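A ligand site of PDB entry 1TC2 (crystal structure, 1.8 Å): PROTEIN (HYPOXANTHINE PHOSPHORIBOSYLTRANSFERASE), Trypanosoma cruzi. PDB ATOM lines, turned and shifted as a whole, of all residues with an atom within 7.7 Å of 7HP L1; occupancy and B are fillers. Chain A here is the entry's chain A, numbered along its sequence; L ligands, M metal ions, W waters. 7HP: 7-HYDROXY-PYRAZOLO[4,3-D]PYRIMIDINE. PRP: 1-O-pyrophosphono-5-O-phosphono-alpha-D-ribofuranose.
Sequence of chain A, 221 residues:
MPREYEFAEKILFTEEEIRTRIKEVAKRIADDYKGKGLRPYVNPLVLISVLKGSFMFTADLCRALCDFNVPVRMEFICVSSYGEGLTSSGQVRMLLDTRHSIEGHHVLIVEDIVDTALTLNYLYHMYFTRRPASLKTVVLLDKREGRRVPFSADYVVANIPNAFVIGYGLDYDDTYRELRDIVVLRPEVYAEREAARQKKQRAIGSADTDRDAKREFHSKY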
ATOM      1  N   ASP A 112     -22.590   1.106  -0.441  1.00  0.00           N
ATOM      2  CA  ASP A 112     -23.109   0.669  -1.729  1.00  0.00           C
ATOM      3  C   ASP A 112     -21.996   0.601  -2.770  1.00  0.00           C
ATOM      4  O   ASP A 112     -21.962  -0.334  -3.572  1.00  0.00           O
ATOM      5  CB  ASP A 112     -24.238   1.591  -2.209  1.00  0.00           C
ATOM      6  CG  ASP A 112     -23.831   3.065  -2.278  1.00  0.00           C
ATOM      7  OD1 ASP A 112     -22.820   3.473  -1.650  1.00  0.00           O
ATOM      8  OD2 ASP A 112     -24.551   3.838  -2.946  1.00  0.00           O
ATOM      9  N   ILE A 113     -21.083   1.566  -2.739  1.00  0.00           N
ATOM     10  CA  ILE A 113     -19.993   1.598  -3.702  1.00  0.00           C
ATOM     11  C   ILE A 113     -18.731   2.270  -3.175  1.00  0.00           C
ATOM     12  O   ILE A 113     -18.785   3.179  -2.331  1.00  0.00           O
ATOM     13  CB  ILE A 113     -20.423   2.259  -5.053  1.00  0.00           C
ATOM     14  CG1 ILE A 113     -19.354   2.031  -6.124  1.00  0.00           C
ATOM     15  CG2 ILE A 113     -20.671   3.750  -4.888  1.00  0.00           C
ATOM     16  CD1 ILE A 113     -19.792   2.377  -7.537  1.00  0.00           C
ATOM     17  N   VAL A 114     -17.580   1.749  -3.595  1.00  0.00           N
ATOM     18  CA  VAL A 114     -16.291   2.334  -3.258  1.00  0.00           C
ATOM     19  C   VAL A 114     -15.575   2.549  -4.573  1.00  0.00           C
ATOM     20  O   VAL A 114     -15.540   1.669  -5.448  1.00  0.00           O
ATOM     21  CB  VAL A 114     -15.477   1.491  -2.236  1.00  0.00           C
ATOM     22  CG1 VAL A 114     -15.122   0.117  -2.791  1.00  0.00           C
ATOM     23  CG2 VAL A 114     -14.261   2.267  -1.781  1.00  0.00           C
ATOM     24  N   ASP A 115     -15.116   3.779  -4.757  1.00  0.00           N
ATOM     25  CA  ASP A 115     -14.430   4.215  -5.966  1.00  0.00           C
ATOM     26  C   ASP A 115     -13.091   4.832  -5.554  1.00  0.00           C
ATOM     27  O   ASP A 115     -12.074   4.113  -5.483  1.00  0.00           O
ATOM     28  CB  ASP A 115     -15.318   5.235  -6.677  1.00  0.00           C
ATOM     29  CG  ASP A 115     -14.744   5.700  -7.991  1.00  0.00           C
ATOM     30  OD1 ASP A 115     -13.830   5.058  -8.529  1.00  0.00           O
ATOM     31  OD2 ASP A 115     -15.261   6.707  -8.519  1.00  0.00           O
ATOM     32  N   THR A 116     -13.087   6.120  -5.214  1.00  0.00           N
ATOM     33  CA  THR A 116     -11.836   6.778  -4.810  1.00  0.00           C
ATOM     34  C   THR A 116     -11.448   6.336  -3.423  1.00  0.00           C
ATOM     35  O   THR A 116     -10.260   6.352  -3.063  1.00  0.00           O
ATOM     36  CB  THR A 116     -11.961   8.296  -4.829  1.00  0.00           C
ATOM     37  OG1 THR A 116     -12.817   8.722  -3.748  1.00  0.00           O
ATOM     38  CG2 THR A 116     -12.529   8.761  -6.169  1.00  0.00           C
ATOM     39  N   LEU A 141     -20.684  -2.725  -4.631  1.00  0.00           N
ATOM     40  CA  LEU A 141     -19.908  -2.588  -5.865  1.00  0.00           C
ATOM     41  C   LEU A 141     -18.539  -1.989  -5.617  1.00  0.00           C
ATOM     42  O   LEU A 141     -18.397  -1.092  -4.781  1.00  0.00           O
ATOM     43  CB  LEU A 141     -20.666  -1.696  -6.849  1.00  0.00           C
ATOM     44  CG  LEU A 141     -22.109  -2.081  -7.191  1.00  0.00           C
ATOM     45  CD1 LEU A 141     -22.713  -1.011  -8.037  1.00  0.00           C
ATOM     46  CD2 LEU A 141     -22.186  -3.416  -7.909  1.00  0.00           C
ATOM     47  N   LYS A 143     -15.199  -0.279  -7.692  1.00  0.00           N
ATOM     48  CA  LYS A 143     -14.497   0.205  -8.881  1.00  0.00           C
ATOM     49  C   LYS A 143     -13.061   0.160  -8.407  1.00  0.00           C
ATOM     50  O   LYS A 143     -12.516   1.163  -7.946  1.00  0.00           O
ATOM     51  CB  LYS A 143     -14.869   1.644  -9.213  1.00  0.00           C
ATOM     52  CG  LYS A 143     -16.219   1.787  -9.835  1.00  0.00           C
ATOM     53  CD  LYS A 143     -16.528   3.232 -10.156  1.00  0.00           C
ATOM     54  CE  LYS A 143     -17.912   3.354 -10.746  1.00  0.00           C
ATOM     55  NZ  LYS A 143     -18.245   4.761 -11.091  1.00  0.00           N
ATOM     56  N   ILE A 160     -16.642  -3.729 -10.554  1.00  0.00           N
ATOM     57  CA  ILE A 160     -17.160  -3.136 -11.770  1.00  0.00           C
ATOM     58  C   ILE A 160     -16.158  -2.142 -12.349  1.00  0.00           C
ATOM     59  O   ILE A 160     -15.246  -1.704 -11.646  1.00  0.00           O
ATOM     60  CB  ILE A 160     -18.520  -2.351 -11.506  1.00  0.00           C
ATOM     61  CG1 ILE A 160     -18.315  -1.276 -10.430  1.00  0.00           C
ATOM     62  CG2 ILE A 160     -19.614  -3.312 -11.082  1.00  0.00           C
ATOM     63  CD1 ILE A 160     -19.360  -0.159 -10.446  1.00  0.00           C
ATOM     64  N   PRO A 161     -16.308  -1.796 -13.643  1.00  0.00           N
ATOM     65  CA  PRO A 161     -15.444  -0.858 -14.367  1.00  0.00           C
ATOM     66  C   PRO A 161     -15.891   0.584 -14.085  1.00  0.00           C
ATOM     67  O   PRO A 161     -16.892   0.807 -13.397  1.00  0.00           O
ATOM     68  CB  PRO A 161     -15.682  -1.231 -15.819  1.00  0.00           C
ATOM     69  CG  PRO A 161     -17.127  -1.641 -15.814  1.00  0.00           C
ATOM     70  CD  PRO A 161     -17.207  -2.503 -14.583  1.00  0.00           C
ATOM     71  N   ASN A 162     -15.182   1.561 -14.636  1.00  0.00           N
ATOM     72  CA  ASN A 162     -15.522   2.955 -14.417  1.00  0.00           C
ATOM     73  C   ASN A 162     -16.699   3.441 -15.240  1.00  0.00           C
ATOM     74  O   ASN A 162     -16.548   4.173 -16.216  1.00  0.00           O
ATOM     75  CB  ASN A 162     -14.319   3.872 -14.654  1.00  0.00           C
ATOM     76  CG  ASN A 162     -14.662   5.348 -14.482  1.00  0.00           C
ATOM     77  OD1 ASN A 162     -14.675   6.132 -15.437  1.00  0.00           O
ATOM     78  ND2 ASN A 162     -14.974   5.735 -13.242  1.00  0.00           N
ATOM     79  N   ALA A 163     -17.887   3.010 -14.863  1.00  0.00           N
ATOM     80  CA  ALA A 163     -19.094   3.427 -15.546  1.00  0.00           C
ATOM     81  C   ALA A 163     -19.889   4.120 -14.458  1.00  0.00           C
ATOM     82  O   ALA A 163     -19.611   3.912 -13.271  1.00  0.00           O
ATOM     83  CB  ALA A 163     -19.855   2.218 -16.054  1.00  0.00           C
ATOM     84  N   PHE A 164     -20.808   5.013 -14.809  1.00  0.00           N
ATOM     85  CA  PHE A 164     -21.637   5.646 -13.780  1.00  0.00           C
ATOM     86  C   PHE A 164     -22.869   4.758 -13.600  1.00  0.00           C
ATOM     87  O   PHE A 164     -23.696   4.668 -14.508  1.00  0.00           O
ATOM     88  CB  PHE A 164     -22.077   7.056 -14.144  1.00  0.00           C
ATOM     89  CG  PHE A 164     -22.562   7.822 -12.962  1.00  0.00           C
ATOM     90  CD1 PHE A 164     -21.653   8.260 -11.983  1.00  0.00           C
ATOM     91  CD2 PHE A 164     -23.915   8.012 -12.731  1.00  0.00           C
ATOM     92  CE1 PHE A 164     -22.094   8.863 -10.799  1.00  0.00           C
ATOM     93  CE2 PHE A 164     -24.369   8.613 -11.549  1.00  0.00           C
ATOM     94  CZ  PHE A 164     -23.456   9.041 -10.580  1.00  0.00           C
ATOM     95  N   VAL A 165     -22.927   4.071 -12.465  1.00  0.00           N
ATOM     96  CA  VAL A 165     -24.055   3.174 -12.162  1.00  0.00           C
ATOM     97  C   VAL A 165     -25.123   3.842 -11.325  1.00  0.00           C
ATOM     98  O   VAL A 165     -24.848   4.773 -10.542  1.00  0.00           O
ATOM     99  CB  VAL A 165     -23.605   1.872 -11.449  1.00  0.00           C
ATOM    100  CG1 VAL A 165     -22.855   0.986 -12.421  1.00  0.00           C
ATOM    101  CG2 VAL A 165     -22.727   2.188 -10.260  1.00  0.00           C
ATOM    102  N   ILE A 166     -26.356   3.370 -11.497  1.00  0.00           N
ATOM    103  CA  ILE A 166     -27.506   3.892 -10.790  1.00  0.00           C
ATOM    104  C   ILE A 166     -28.464   2.749 -10.511  1.00  0.00           C
ATOM    105  O   ILE A 166     -28.469   1.730 -11.216  1.00  0.00           O
ATOM    106  CB  ILE A 166     -28.243   4.980 -11.617  1.00  0.00           C
ATOM    107  CG1 ILE A 166     -28.421   4.492 -13.046  1.00  0.00           C
ATOM    108  CG2 ILE A 166     -27.503   6.298 -11.572  1.00  0.00           C
ATOM    109  CD1 ILE A 166     -29.329   5.350 -13.883  1.00  0.00           C
ATOM    110  N   GLY A 167     -29.287   2.944  -9.478  1.00  0.00           N
ATOM    111  CA  GLY A 167     -30.244   1.939  -9.098  1.00  0.00           C
ATOM    112  C   GLY A 167     -29.794   1.278  -7.827  1.00  0.00           C
ATOM    113  O   GLY A 167     -28.639   1.458  -7.399  1.00  0.00           O
ATOM    114  N   GLY A 169     -30.305   1.906  -4.691  1.00  0.00           N
ATOM    115  CA  GLY A 169     -29.784   2.832  -3.702  1.00  0.00           C
ATOM    116  C   GLY A 169     -28.889   3.899  -4.290  1.00  0.00           C
ATOM    117  O   GLY A 169     -28.803   5.000  -3.761  1.00  0.00           O
ATOM    118  N   LEU A 170     -28.211   3.567  -5.380  1.00  0.00           N
ATOM    119  CA  LEU A 170     -27.296   4.472  -6.077  1.00  0.00           C
ATOM    120  C   LEU A 170     -28.000   5.505  -6.938  1.00  0.00           C
ATOM    121  O   LEU A 170     -28.790   5.164  -7.816  1.00  0.00           O
ATOM    122  CB  LEU A 170     -26.369   3.657  -6.981  1.00  0.00           C
ATOM    123  CG  LEU A 170     -25.408   2.755  -6.236  1.00  0.00           C
ATOM    124  CD1 LEU A 170     -25.223   1.500  -7.023  1.00  0.00           C
ATOM    125  CD2 LEU A 170     -24.081   3.467  -6.023  1.00  0.00           C
ATOM    126  N   ASP A 171     -27.566   6.753  -6.833  1.00  0.00           N
ATOM    127  CA  ASP A 171     -28.196   7.809  -7.598  1.00  0.00           C
ATOM    128  C   ASP A 171     -27.303   8.613  -8.515  1.00  0.00           C
ATOM    129  O   ASP A 171     -26.070   8.580  -8.444  1.00  0.00           O
ATOM    130  CB  ASP A 171     -28.775   8.840  -6.643  1.00  0.00           C
ATOM    131  CG  ASP A 171     -27.690   9.679  -5.974  1.00  0.00           C
ATOM    132  OD1 ASP A 171     -26.821   9.094  -5.270  1.00  0.00           O
ATOM    133  OD2 ASP A 171     -27.688  10.916  -6.176  1.00  0.00           O
ATOM    134  N   TYR A 172     -27.985   9.446  -9.288  1.00  0.00           N
ATOM    135  CA  TYR A 172     -27.370  10.445 -10.127  1.00  0.00           C
ATOM    136  C   TYR A 172     -28.299  11.624  -9.828  1.00  0.00           C
ATOM    137  O   TYR A 172     -29.502  11.547 -10.082  1.00  0.00           O
ATOM    138  CB  TYR A 172     -27.441  10.146 -11.618  1.00  0.00           C
ATOM    139  CG  TYR A 172     -27.200  11.433 -12.384  1.00  0.00           C
ATOM    140  CD1 TYR A 172     -26.028  12.168 -12.190  1.00  0.00           C
ATOM    141  CD2 TYR A 172     -28.190  11.980 -13.202  1.00  0.00           C
ATOM    142  CE1 TYR A 172     -25.857  13.427 -12.782  1.00  0.00           C
ATOM    143  CE2 TYR A 172     -28.032  13.231 -13.790  1.00  0.00           C
ATOM    144  CZ  TYR A 172     -26.871  13.949 -13.571  1.00  0.00           C
ATOM    145  OH  TYR A 172     -26.728  15.190 -14.155  1.00  0.00           O
ATOM    146  N   ARG A 177     -32.526   6.095  -7.309  1.00  0.00           N
ATOM    147  CA  ARG A 177     -32.132   5.238  -6.199  1.00  0.00           C
ATOM    148  C   ARG A 177     -33.068   4.046  -6.033  1.00  0.00           C
ATOM    149  O   ARG A 177     -32.664   2.980  -5.570  1.00  0.00           O
ATOM    150  CB  ARG A 177     -32.134   5.989  -4.867  1.00  0.00           C
ATOM    151  CG  ARG A 177     -31.283   7.220  -4.785  1.00  0.00           C
ATOM    152  CD  ARG A 177     -31.061   7.570  -3.315  1.00  0.00           C
ATOM    153  NE  ARG A 177     -30.341   8.827  -3.178  1.00  0.00           N
ATOM    154  CZ  ARG A 177     -29.016   8.928  -3.071  1.00  0.00           C
ATOM    155  NH1 ARG A 177     -28.251   7.838  -3.080  1.00  0.00           N
ATOM    156  NH2 ARG A 177     -28.466  10.131  -3.039  1.00  0.00           N
ATOM    157  N   VAL A 183     -27.992  -0.347 -13.144  1.00  0.00           N
ATOM    158  CA  VAL A 183     -27.780  -0.073 -14.557  1.00  0.00           C
ATOM    159  C   VAL A 183     -26.732   1.049 -14.738  1.00  0.00           C
ATOM    160  O   VAL A 183     -26.303   1.697 -13.769  1.00  0.00           O
ATOM    161  CB  VAL A 183     -29.148   0.341 -15.244  1.00  0.00           C
ATOM    162  CG1 VAL A 183     -30.222  -0.728 -15.001  1.00  0.00           C
ATOM    163  CG2 VAL A 183     -29.625   1.699 -14.727  1.00  0.00           C
ATOM    164  N   LEU A 185     -25.850   4.593 -16.360  1.00  0.00           N
ATOM    165  CA  LEU A 185     -26.505   5.804 -16.844  1.00  0.00           C
ATOM    166  C   LEU A 185     -25.984   6.163 -18.221  1.00  0.00           C
ATOM    167  O   LEU A 185     -24.777   6.162 -18.452  1.00  0.00           O
ATOM    168  CB  LEU A 185     -26.266   6.957 -15.872  1.00  0.00           C
ATOM    169  CG  LEU A 185     -26.960   8.286 -16.140  1.00  0.00           C
ATOM    170  CD1 LEU A 185     -28.491   8.140 -16.047  1.00  0.00           C
ATOM    171  CD2 LEU A 185     -26.470   9.316 -15.137  1.00  0.00           C
HETATM  172  C9  7HP L   1     -20.225   7.263  -6.586  1.00  0.00           C
HETATM  173  C4  7HP L   1     -21.266   6.845  -7.405  1.00  0.00           C
HETATM  174  N3  7HP L   1     -22.592   7.031  -7.190  1.00  0.00           N
HETATM  175  C2  7HP L   1     -23.327   6.423  -8.176  1.00  0.00           C
HETATM  176  N1  7HP L   1     -22.764   5.757  -9.245  1.00  0.00           N
HETATM  177  C6  7HP L   1     -21.427   5.597  -9.463  1.00  0.00           C
HETATM  178  O6  7HP L   1     -21.019   5.059 -10.480  1.00  0.00           O
HETATM  179  C5  7HP L   1     -20.676   6.184  -8.468  1.00  0.00           C
HETATM  180  N7  7HP L   1     -19.316   6.231  -8.284  1.00  0.00           N
HETATM  181  N8  7HP L   1     -19.129   6.872  -7.176  1.00  0.00           N
HETATM  182  C1  PRP L   2     -21.394   7.940  -3.021  1.00  0.00           C
HETATM  183  C2  PRP L   2     -21.645   6.463  -2.776  1.00  0.00           C
HETATM  184  C3  PRP L   2     -20.497   6.172  -1.774  1.00  0.00           C
HETATM  185  C4  PRP L   2     -19.366   7.068  -2.352  1.00  0.00           C
HETATM  186  C5  PRP L   2     -18.517   6.202  -3.323  1.00  0.00           C
HETATM  187  O1  PRP L   2     -22.015   8.706  -1.945  1.00  0.00           O
HETATM  188  O2  PRP L   2     -23.010   6.302  -2.216  1.00  0.00           O
HETATM  189  O3  PRP L   2     -20.701   6.607  -0.439  1.00  0.00           O
HETATM  190  O4  PRP L   2     -19.999   8.170  -3.047  1.00  0.00           O
HETATM  191  O5  PRP L   2     -17.461   6.896  -4.042  1.00  0.00           O
HETATM  192  P   PRP L   2     -15.926   7.287  -3.454  1.00  0.00           P
HETATM  193  O1P PRP L   2     -15.284   6.000  -3.012  1.00  0.00           O
HETATM  194  O2P PRP L   2     -16.198   8.164  -2.286  1.00  0.00           O
HETATM  195  O3P PRP L   2     -15.315   7.976  -4.637  1.00  0.00           O
HETATM  196  PA  PRP L   2     -22.664  10.186  -2.206  1.00  0.00           P
HETATM  197  O1A PRP L   2     -21.672  11.235  -1.967  1.00  0.00           O
HETATM  198  O2A PRP L   2     -23.109  10.191  -3.609  1.00  0.00           O
HETATM  199  O3A PRP L   2     -23.799  10.166  -1.222  1.00  0.00           O
HETATM  200  PB  PRP L   2     -25.077   9.361  -1.298  1.00  0.00           P
HETATM  201  O1B PRP L   2     -25.624   9.309  -2.695  1.00  0.00           O
HETATM  202  O2B PRP L   2     -26.061   9.959  -0.423  1.00  0.00           O
HETATM  203  O3B PRP L   2     -24.858   8.000  -0.770  1.00  0.00           O
HETATM  204 MG    MG M   1     -24.863   9.751  -4.673  1.00  0.00          MG
HETATM  205 MG    MG M   2     -22.923   7.109  -0.222  1.00  0.00          MG
HETATM  206  O   HOH W   1     -24.313   7.816  -4.858  1.00  0.00           O
HETATM  207  O   HOH W   2     -16.552   8.483  -6.815  1.00  0.00           O
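O6 of 7HP L1 sits at hydrogen-bond distance from N of Val 165, at 2.9 Å. The backbone carbonyl oxygen of Val 165 sits close to a nitrogen (N1) of 7HP L1, at 2.6 Å. O6 of 7HP L1 lies within hydrogen-bond range of NZ of Lys 143 (2.9 Å). The backbone carbonyl oxygen (O) of Ala 163 is in hydrogen-bond range of an oxygen (O6) of 7HP L1. The backbone NH (N) of Asp 115 sits at hydrogen-bond distance from an oxygen (O1P) of PRP L2 (2.8 Å). OD1 of Asp 112 lies close to O2 of PRP L2 (2.9 Å). N of Thr 116 is in hydrogen-bond range of O3P of PRP L2 (3.0 Å). The side-chain hydroxyl (OG1) of Thr 116 is in hydrogen-bond range of an oxygen (O3P) of PRP L2 (2.8 Å). The guanidinium group (NH2) of Arg 177 is in salt-bridge range of an oxygen (O2B) of PRP L2 (3.6 Å).
Water W2 lies within hydrogen-bond range of O3P of PRP L2 (2.6 Å), OD2 of Asp 115 (2.8 Å) and N8 of 7HP L1 (3.1 Å).
NZ of Lys 143 lies within hydrogen-bond range of O of Ala 163 (2.7 Å). The backbone NH (N) of Lys 143 sits at hydrogen-bond distance from the backbone carbonyl oxygen (O) of Val 114 (3.0 Å). O of Phe 164 lies within hydrogen-bond range of N of Leu 185 (2.8 Å). The side-chain carboxylate of Asp 171 is in salt-bridge range of the guanidinium group of Arg 177 (3.3 Å).
Ile 113 touches 7HP L1. CA of Phe 164 touches O6 of 7HP L1, 3.4 Å away. Leu 170 touches 7HP L1 (CD2 to C2, 3.7 Å). O of Asp 171 touches C2 of 7HP L1, at 3.5 Å. Hydrophobic or aromatic side chains that line 7HP L1: Ile 113, Phe 164, Val 165 and Leu 170. The nearest printed residue that does not touch 7HP L1 is Asp 115 (4.1 Å).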
